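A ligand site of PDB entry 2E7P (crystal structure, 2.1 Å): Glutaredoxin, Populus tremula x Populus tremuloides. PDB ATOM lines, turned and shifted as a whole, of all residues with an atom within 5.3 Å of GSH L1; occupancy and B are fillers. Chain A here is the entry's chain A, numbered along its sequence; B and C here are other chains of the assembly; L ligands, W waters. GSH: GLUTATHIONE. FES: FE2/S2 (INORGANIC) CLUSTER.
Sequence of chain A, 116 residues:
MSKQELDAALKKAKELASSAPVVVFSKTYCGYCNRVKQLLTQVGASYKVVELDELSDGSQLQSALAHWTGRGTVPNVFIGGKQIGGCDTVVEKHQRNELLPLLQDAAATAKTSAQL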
ATOM      1  N   LYS A  27      24.413  13.726  -1.733  1.00  0.00           N
ATOM      2  CA  LYS A  27      25.423  13.416  -0.765  1.00  0.00           C
ATOM      3  C   LYS A  27      26.767  13.884  -1.344  1.00  0.00           C
ATOM      4  O   LYS A  27      27.028  13.712  -2.549  1.00  0.00           O
ATOM      5  CB  LYS A  27      25.426  11.941  -0.401  1.00  0.00           C
ATOM      6  CG  LYS A  27      24.134  11.482   0.302  1.00  0.00           C
ATOM      7  CD  LYS A  27      24.186  10.024   0.752  1.00  0.00           C
ATOM      8  CE  LYS A  27      22.802   9.606   1.287  1.00  0.00           C
ATOM      9  NZ  LYS A  27      22.747   8.180   1.769  1.00  0.00           N
ATOM     10  N   TYR A  29      29.832  13.115  -1.409  1.00  0.00           N
ATOM     11  CA  TYR A  29      30.794  12.187  -2.014  1.00  0.00           C
ATOM     12  C   TYR A  29      30.351  11.591  -3.339  1.00  0.00           C
ATOM     13  O   TYR A  29      31.214  11.084  -4.065  1.00  0.00           O
ATOM     14  CB  TYR A  29      31.165  11.058  -1.002  1.00  0.00           C
ATOM     15  CG  TYR A  29      29.991  10.247  -0.544  1.00  0.00           C
ATOM     16  CD1 TYR A  29      29.457   9.253  -1.358  1.00  0.00           C
ATOM     17  CD2 TYR A  29      29.382  10.467   0.723  1.00  0.00           C
ATOM     18  CE1 TYR A  29      28.338   8.500  -0.952  1.00  0.00           C
ATOM     19  CE2 TYR A  29      28.273   9.736   1.130  1.00  0.00           C
ATOM     20  CZ  TYR A  29      27.761   8.755   0.298  1.00  0.00           C
ATOM     21  OH  TYR A  29      26.682   7.976   0.669  1.00  0.00           O
ATOM     22  N   CYS A  30      29.036  11.645  -3.652  1.00  0.00           N
ATOM     23  CA  CYS A  30      28.410  10.906  -4.778  1.00  0.00           C
ATOM     24  C   CYS A  30      28.660  11.484  -6.174  1.00  0.00           C
ATOM     25  O   CYS A  30      28.232  12.591  -6.507  1.00  0.00           O
ATOM     26  CB  CYS A  30      26.893  10.668  -4.624  1.00  0.00           C
ATOM     27  SG  CYS A  30      26.297   9.378  -5.816  1.00  0.00           S
ATOM     28  N   TYR A  32      27.182  10.497  -8.909  1.00  0.00           N
ATOM     29  CA  TYR A  32      25.913  10.784  -9.639  1.00  0.00           C
ATOM     30  C   TYR A  32      25.356  12.153  -9.265  1.00  0.00           C
ATOM     31  O   TYR A  32      24.784  12.887 -10.101  1.00  0.00           O
ATOM     32  CB  TYR A  32      24.826   9.731  -9.365  1.00  0.00           C
ATOM     33  CG  TYR A  32      24.942   8.494 -10.227  1.00  0.00           C
ATOM     34  CD1 TYR A  32      25.049   8.605 -11.620  1.00  0.00           C
ATOM     35  CD2 TYR A  32      24.933   7.246  -9.666  1.00  0.00           C
ATOM     36  CE1 TYR A  32      25.162   7.483 -12.429  1.00  0.00           C
ATOM     37  CE2 TYR A  32      25.034   6.103 -10.462  1.00  0.00           C
ATOM     38  CZ  TYR A  32      25.140   6.236 -11.835  1.00  0.00           C
ATOM     39  OH  TYR A  32      25.251   5.114 -12.630  1.00  0.00           O
ATOM     40  N   GLN A  62      15.691  11.120   3.981  1.00  0.00           N
ATOM     41  CA  GLN A  62      15.605  10.208   2.808  1.00  0.00           C
ATOM     42  C   GLN A  62      14.362   9.329   2.819  1.00  0.00           C
ATOM     43  O   GLN A  62      13.782   9.093   1.750  1.00  0.00           O
ATOM     44  CB  GLN A  62      16.819   9.274   2.696  1.00  0.00           C
ATOM     45  CG  GLN A  62      18.109   9.917   2.279  1.00  0.00           C
ATOM     46  CD  GLN A  62      19.163   8.877   1.980  1.00  0.00           C
ATOM     47  OE1 GLN A  62      19.050   8.108   1.019  1.00  0.00           O
ATOM     48  NE2 GLN A  62      20.194   8.837   2.826  1.00  0.00           N
ATOM     49  N   ARG A  71      11.118   8.408  -4.327  1.00  0.00           N
ATOM     50  CA  ARG A  71      12.565   8.330  -4.551  1.00  0.00           C
ATOM     51  C   ARG A  71      13.269   8.496  -3.244  1.00  0.00           C
ATOM     52  O   ARG A  71      13.219   9.564  -2.630  1.00  0.00           O
ATOM     53  CB  ARG A  71      13.044   9.415  -5.522  1.00  0.00           C
ATOM     54  CG  ARG A  71      14.560   9.445  -5.718  1.00  0.00           C
ATOM     55  CD  ARG A  71      14.981  10.408  -6.808  1.00  0.00           C
ATOM     56  NE  ARG A  71      14.296  10.117  -8.064  1.00  0.00           N
ATOM     57  CZ  ARG A  71      14.785   9.325  -9.011  1.00  0.00           C
ATOM     58  NH1 ARG A  71      15.966   8.742  -8.863  1.00  0.00           N
ATOM     59  NH2 ARG A  71      14.070   9.131 -10.118  1.00  0.00           N
ATOM     60  N   GLY A  72      13.952   7.426  -2.814  1.00  0.00           N
ATOM     61  CA  GLY A  72      14.764   7.484  -1.585  1.00  0.00           C
ATOM     62  C   GLY A  72      16.260   7.636  -1.868  1.00  0.00           C
ATOM     63  O   GLY A  72      17.071   7.775  -0.929  1.00  0.00           O
ATOM     64  N   THR A  73      16.636   7.626  -3.140  1.00  0.00           N
ATOM     65  CA  THR A  73      18.055   7.756  -3.513  1.00  0.00           C
ATOM     66  C   THR A  73      18.472   9.197  -3.807  1.00  0.00           C
ATOM     67  O   THR A  73      17.618  10.082  -3.927  1.00  0.00           O
ATOM     68  CB  THR A  73      18.402   6.906  -4.733  1.00  0.00           C
ATOM     69  OG1 THR A  73      17.610   7.330  -5.843  1.00  0.00           O
ATOM     70  CG2 THR A  73      18.195   5.396  -4.424  1.00  0.00           C
ATOM     71  N   VAL A  74      19.773   9.428  -3.882  1.00  0.00           N
ATOM     72  CA  VAL A  74      20.287  10.701  -4.345  1.00  0.00           C
ATOM     73  C   VAL A  74      21.016  10.499  -5.701  1.00  0.00           C
ATOM     74  O   VAL A  74      21.571   9.434  -5.952  1.00  0.00           O
ATOM     75  CB  VAL A  74      21.183  11.375  -3.308  1.00  0.00           C
ATOM     76  CG1 VAL A  74      20.405  11.664  -2.035  1.00  0.00           C
ATOM     77  CG2 VAL A  74      22.394  10.474  -2.977  1.00  0.00           C
ATOM     78  N   PRO A  75      21.035  11.551  -6.575  1.00  0.00           N
ATOM     79  CA  PRO A  75      20.431  12.863  -6.292  1.00  0.00           C
ATOM     80  C   PRO A  75      18.900  12.815  -6.442  1.00  0.00           C
ATOM     81  O   PRO A  75      18.368  11.951  -7.161  1.00  0.00           O
ATOM     82  CB  PRO A  75      21.057  13.797  -7.347  1.00  0.00           C
ATOM     83  CG  PRO A  75      21.487  12.886  -8.500  1.00  0.00           C
ATOM     84  CD  PRO A  75      21.642  11.468  -7.920  1.00  0.00           C
ATOM     85  N   GLY A  86      16.147  11.963 -10.554  1.00  0.00           N
ATOM     86  CA  GLY A  86      17.536  11.714 -10.178  1.00  0.00           C
ATOM     87  C   GLY A  86      18.467  12.037 -11.330  1.00  0.00           C
ATOM     88  O   GLY A  86      18.117  12.788 -12.251  1.00  0.00           O
ATOM     89  N   CYS A  87      19.657  11.466 -11.303  1.00  0.00           N
ATOM     90  CA  CYS A  87      20.692  11.835 -12.252  1.00  0.00           C
ATOM     91  C   CYS A  87      20.269  11.452 -13.662  1.00  0.00           C
ATOM     92  O   CYS A  87      20.229  12.308 -14.551  1.00  0.00           O
ATOM     93  CB  CYS A  87      22.043  11.199 -11.902  1.00  0.00           C
ATOM     94  SG  CYS A  87      23.329  11.714 -13.060  1.00  0.00           S
ATOM     95  N   ASP A  88      19.955  10.169 -13.860  1.00  0.00           N
ATOM     96  CA  ASP A  88      19.427   9.672 -15.146  1.00  0.00           C
ATOM     97  C   ASP A  88      18.290  10.529 -15.707  1.00  0.00           C
ATOM     98  O   ASP A  88      18.283  10.808 -16.881  1.00  0.00           O
ATOM     99  CB  ASP A  88      18.945   8.213 -15.063  1.00  0.00           C
ATOM    100  CG  ASP A  88      20.064   7.226 -14.823  1.00  0.00           C
ATOM    101  OD1 ASP A  88      21.246   7.588 -15.016  1.00  0.00           O
ATOM    102  OD2 ASP A  88      19.760   6.059 -14.444  1.00  0.00           O
ATOM    103  N   THR A  89      17.309  10.898 -14.880  1.00  0.00           N
ATOM    104  CA  THR A  89      16.154  11.676 -15.361  1.00  0.00           C
ATOM    105  C   THR A  89      16.585  13.016 -15.942  1.00  0.00           C
ATOM    106  O   THR A  89      16.165  13.393 -17.032  1.00  0.00           O
ATOM    107  CB  THR A  89      15.132  12.018 -14.239  1.00  0.00           C
ATOM    108  OG1 THR A  89      14.809  10.844 -13.497  1.00  0.00           O
ATOM    109  CG2 THR A  89      13.827  12.584 -14.830  1.00  0.00           C
ATOM    110  N   TYR B  29      28.410   1.399  -1.107  1.00  0.00           N
ATOM    111  CA  TYR B  29      27.486   2.515  -1.227  1.00  0.00           C
ATOM    112  C   TYR B  29      27.444   3.190  -2.611  1.00  0.00           C
ATOM    113  O   TYR B  29      26.628   4.097  -2.813  1.00  0.00           O
ATOM    114  CB  TYR B  29      27.808   3.550  -0.135  1.00  0.00           C
ATOM    115  CG  TYR B  29      29.228   4.062  -0.180  1.00  0.00           C
ATOM    116  CD1 TYR B  29      29.619   5.008  -1.145  1.00  0.00           C
ATOM    117  CD2 TYR B  29      30.188   3.584   0.723  1.00  0.00           C
ATOM    118  CE1 TYR B  29      30.911   5.474  -1.203  1.00  0.00           C
ATOM    119  CE2 TYR B  29      31.508   4.047   0.684  1.00  0.00           C
ATOM    120  CZ  TYR B  29      31.858   4.983  -0.287  1.00  0.00           C
ATOM    121  OH  TYR B  29      33.140   5.418  -0.331  1.00  0.00           O
ATOM    122  N   CYS B  30      28.298   2.787  -3.565  1.00  0.00           N
ATOM    123  CA  CYS B  30      28.446   3.575  -4.772  1.00  0.00           C
ATOM    124  C   CYS B  30      27.649   3.072  -5.965  1.00  0.00           C
ATOM    125  O   CYS B  30      27.838   1.960  -6.432  1.00  0.00           O
ATOM    126  CB  CYS B  30      29.926   3.796  -5.182  1.00  0.00           C
ATOM    127  SG  CYS B  30      30.133   5.108  -6.495  1.00  0.00           S
ATOM    128  N   GLY B  31      26.839   3.964  -6.516  1.00  0.00           N
ATOM    129  CA  GLY B  31      26.058   3.700  -7.710  1.00  0.00           C
ATOM    130  C   GLY B  31      26.882   3.515  -8.951  1.00  0.00           C
ATOM    131  O   GLY B  31      26.501   2.741  -9.820  1.00  0.00           O
ATOM    132  N   TYR B  32      28.004   4.218  -9.075  1.00  0.00           N
ATOM    133  CA  TYR B  32      28.916   3.978 -10.191  1.00  0.00           C
ATOM    134  C   TYR B  32      29.406   2.545 -10.143  1.00  0.00           C
ATOM    135  O   TYR B  32      29.445   1.854 -11.155  1.00  0.00           O
ATOM    136  CB  TYR B  32      30.103   4.951 -10.158  1.00  0.00           C
ATOM    137  CG  TYR B  32      29.822   6.344 -10.744  1.00  0.00           C
ATOM    138  CD1 TYR B  32      28.738   6.548 -11.563  1.00  0.00           C
ATOM    139  CD2 TYR B  32      30.650   7.449 -10.460  1.00  0.00           C
ATOM    140  CE1 TYR B  32      28.452   7.791 -12.100  1.00  0.00           C
ATOM    141  CE2 TYR B  32      30.401   8.697 -11.013  1.00  0.00           C
ATOM    142  CZ  TYR B  32      29.270   8.851 -11.837  1.00  0.00           C
ATOM    143  OH  TYR B  32      28.931  10.057 -12.453  1.00  0.00           O
ATOM    144  N   THR C  73      15.623   1.559  -1.903  1.00  0.00           N
ATOM    145  CA  THR C  73      16.643   0.660  -2.407  1.00  0.00           C
ATOM    146  C   THR C  73      16.164  -0.805  -2.425  1.00  0.00           C
ATOM    147  O   THR C  73      15.172  -1.167  -1.769  1.00  0.00           O
ATOM    148  CB  THR C  73      17.919   0.754  -1.526  1.00  0.00           C
ATOM    149  OG1 THR C  73      17.599   0.425  -0.159  1.00  0.00           O
ATOM    150  CG2 THR C  73      18.570   2.146  -1.578  1.00  0.00           C
HETATM  151  N1  GSH L   1      19.141   5.829 -11.107  1.00  0.00           N
HETATM  152  CA1 GSH L   1      19.541   6.714 -10.038  1.00  0.00           C
HETATM  153  C1  GSH L   1      19.763   8.083 -10.626  1.00  0.00           C
HETATM  154  O11 GSH L   1      19.856   9.086  -9.900  1.00  0.00           O
HETATM  155  O12 GSH L   1      19.781   8.139 -11.845  1.00  0.00           O
HETATM  156  CB1 GSH L   1      20.801   6.208  -9.329  1.00  0.00           C
HETATM  157  CG1 GSH L   1      20.850   6.783  -7.932  1.00  0.00           C
HETATM  158  CD1 GSH L   1      21.669   5.985  -6.960  1.00  0.00           C
HETATM  159  OE1 GSH L   1      21.936   4.805  -7.182  1.00  0.00           O
HETATM  160  N2  GSH L   1      22.037   6.651  -5.858  1.00  0.00           N
HETATM  161  CA2 GSH L   1      22.833   6.049  -4.812  1.00  0.00           C
HETATM  162  C2  GSH L   1      22.028   6.027  -3.517  1.00  0.00           C
HETATM  163  O2  GSH L   1      21.277   6.954  -3.221  1.00  0.00           O
HETATM  164  CB2 GSH L   1      24.213   6.792  -4.680  1.00  0.00           C
HETATM  165  SG2 GSH L   1      25.526   6.956  -5.955  1.00  0.00           S
HETATM  166  N3  GSH L   1      22.131   4.964  -2.702  1.00  0.00           N
HETATM  167  CA3 GSH L   1      21.400   4.791  -1.438  1.00  0.00           C
HETATM  168  C3  GSH L   1      21.745   5.780  -0.339  1.00  0.00           C
HETATM  169  O31 GSH L   1      22.774   6.496  -0.451  1.00  0.00           O
HETATM  170  O32 GSH L   1      21.018   5.835   0.686  1.00  0.00           O
HETATM  171 FE1  FES L   2      29.539   6.719  -6.345  1.00  0.00          FE
HETATM  172 FE2  FES L   2      27.001   7.818  -5.842  1.00  0.00          FE
HETATM  173  S1  FES L   2      28.430   7.262  -5.166  1.00  0.00           S
HETATM  174  S2  FES L   2      28.091   7.320  -7.190  1.00  0.00           S
HETATM  175  N1  GSH L   3      21.534  -0.643   3.167  1.00  0.00           N
HETATM  176  CA1 GSH L   3      20.689  -1.137   2.080  1.00  0.00           C
HETATM  177  C1  GSH L   3      20.406  -2.582   2.367  1.00  0.00           C
HETATM  178  O11 GSH L   3      19.592  -3.253   1.695  1.00  0.00           O
HETATM  179  O12 GSH L   3      21.056  -3.099   3.300  1.00  0.00           O
HETATM  180  CB1 GSH L   3      21.514  -1.000   0.783  1.00  0.00           C
HETATM  181  CG1 GSH L   3      20.843  -1.456  -0.535  1.00  0.00           C
HETATM  182  CD1 GSH L   3      21.460  -0.793  -1.774  1.00  0.00           C
HETATM  183  OE1 GSH L   3      22.394   0.004  -1.660  1.00  0.00           O
HETATM  184  N2  GSH L   3      20.971  -1.122  -2.974  1.00  0.00           N
HETATM  185  CA2 GSH L   3      21.402  -0.507  -4.220  1.00  0.00           C
HETATM  186  C2  GSH L   3      20.232   0.310  -4.698  1.00  0.00           C
HETATM  187  O2  GSH L   3      19.109  -0.089  -4.465  1.00  0.00           O
HETATM  188  CB2 GSH L   3      21.579  -1.592  -5.256  1.00  0.00           C
HETATM  189  SG2 GSH L   3      23.054  -2.563  -4.922  1.00  0.00           S
HETATM  190  N3  GSH L   3      20.417   1.427  -5.418  1.00  0.00           N
HETATM  191  CA3 GSH L   3      19.348   2.258  -5.959  1.00  0.00           C
HETATM  192  C3  GSH L   3      18.650   1.573  -7.121  1.00  0.00           C
HETATM  193  O31 GSH L   3      19.068   0.477  -7.580  1.00  0.00           O
HETATM  194  O32 GSH L   3      17.654   2.105  -7.638  1.00  0.00           O
HETATM  195  O   HOH W   1      17.041   9.251 -12.545  1.00  0.00           O
HETATM  196  O   HOH W   2      17.050   5.376 -13.822  1.00  0.00           O
HETATM  197  O   HOH W   3      24.195   3.303  -3.719  1.00  0.00           O
HETATM  198  O   HOH W   4      19.629   3.103 -10.855  1.00  0.00           O
HETATM  199  O   HOH W   5      23.187   2.502  -5.881  1.00  0.00           O
HETATM  200  O   HOH W   6      16.596   6.364 -11.299  1.00  0.00           O
HETATM  201  O   HOH W   7      25.401   6.272  -1.105  1.00  0.00           O
HETATM  202  O   HOH W   8      21.921   2.766  -8.984  1.00  0.00           O
HETATM  203  O   HOH W   9      18.367   9.420  -7.649  1.00  0.00           O
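The side-chain amino group of Lys 27 lies close to the side-chain amide nitrogen of Gln 62.
SG of Cys 87 sits at hydrogen-bond distance from O of Tyr 32 of chain A (3.5 Å).
The backbone NH (N) of Gly 86 sits at hydrogen-bond distance from the side-chain hydroxyl (OG1) of Thr 89 (3.4 Å).
The side-chain amide oxygen of Gln 62 lies close to the backbone carbonyl oxygen of Gly 72 (2.8 Å).
The side-chain sulfur of Cys 30 of chain A lies close to the backbone NH of Tyr 32 of chain A (3.4 Å).
SG2 of GSH L1 is bound to FE2 of FES L2 (1.7 Å).
Water W6 bridges N1 of GSH L1 (2.6 Å) and NH1 of Arg 71 (3.5 Å).
Water W7 lies within hydrogen-bond range of an oxygen (O31) of GSH L1 (2.7 Å), the side-chain hydroxyl of Tyr 29 of chain A (2.8 Å) and the backbone carbonyl oxygen of Tyr 29 of chain B (3.0 Å).
Water W9 lies within hydrogen-bond range of O of Pro 75 (2.6 Å), O11 of GSH L1 (2.7 Å), NH1 of Arg 71 (2.8 Å) and OG1 of Thr 73 of chain A (2.9 Å).
Water W3 lies within hydrogen-bond range of the backbone carbonyl oxygen (O) of Tyr 29 of chain B (2.7 Å) and a nitrogen (N3) of GSH L1 (2.8 Å).
Water W5 lies within hydrogen-bond range of an oxygen (OE1) of GSH L1 (2.9 Å) and a nitrogen (N3) of GSH L3 (3.0 Å).
Water W2 bridges the side-chain carboxylate of Asp 88 (2.9 Å) and a nitrogen (N1) of GSH L1 (3.5 Å).
O of Val 74 lies within hydrogen-bond range of N2 of GSH L1, at 2.8 Å.
The side-chain sulfur of Cys 30 of chain A binds an iron atom (FE2) of FES L2 (1.7 Å).
An oxygen (O32) of GSH L1 sits close to the side-chain amide oxygen of Gln 62.
N of Asp 88 is in hydrogen-bond range of O12 of GSH L1, at 2.9 Å.
The backbone NH (N) of Cys 87 sits at hydrogen-bond distance from an oxygen (O11) of GSH L1 (2.8 Å).
A sulfur (S2) of FES L2 lies close to the backbone NH of Gly 31 of chain B.
SG of Cys 30 of chain B binds FE1 of FES L2 (1.7 Å).
The side-chain amino group (NZ) of Lys 27 is in salt-bridge range of an oxygen (O31) of GSH L1, at 2.8 Å.
The backbone NH (N) of Tyr 32 of chain B lies close to a sulfur (S2) of FES L2.
The backbone NH (N) of Tyr 32 of chain A lies close to a sulfur (S2) of FES L2 (3.7 Å).
The backbone NH (N) of Gly 31 of chain B sits close to a sulfur (SG2) of GSH L1, at 3.3 Å.
The backbone NH of Val 74 sits at hydrogen-bond distance from an oxygen (O2) of GSH L1, at 3.0 Å.
OD2 of Asp 88 lies within salt-bridge range of N1 of GSH L1, at 3.4 Å.
The side-chain sulfur of Cys 30 of chain A sits close to a sulfur (SG2) of GSH L1 (2.5 Å).
Tyr 32 of chain A touches GSH L1 (CD2 to SG2, 3.8 Å).
CB of Thr 73 of chain A touches O2 of GSH L1, 3.2 Å away.
Pro 75 touches GSH L1 (CD to O11, 3.6 Å).
Gly 86 touches GSH L1 (CA to O11, 3.5 Å).
Thr 73 of chain C touches GSH L1 (CG2 to CA3, 3.9 Å).
Hydrophobic or aromatic side chains within 4 Å of GSH L1: Tyr 32 of chain A, Val 74 and Pro 75.
Within 4 Å of GSH L1: Lys 27, Cys 30 of chain A, Tyr 32 of chain A, Gln 62, Thr 73 of chain A, Val 74, Pro 75, Gly 86, Cys 87, Asp 88, Gly 31 of chain B and Thr 73 of chain C.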
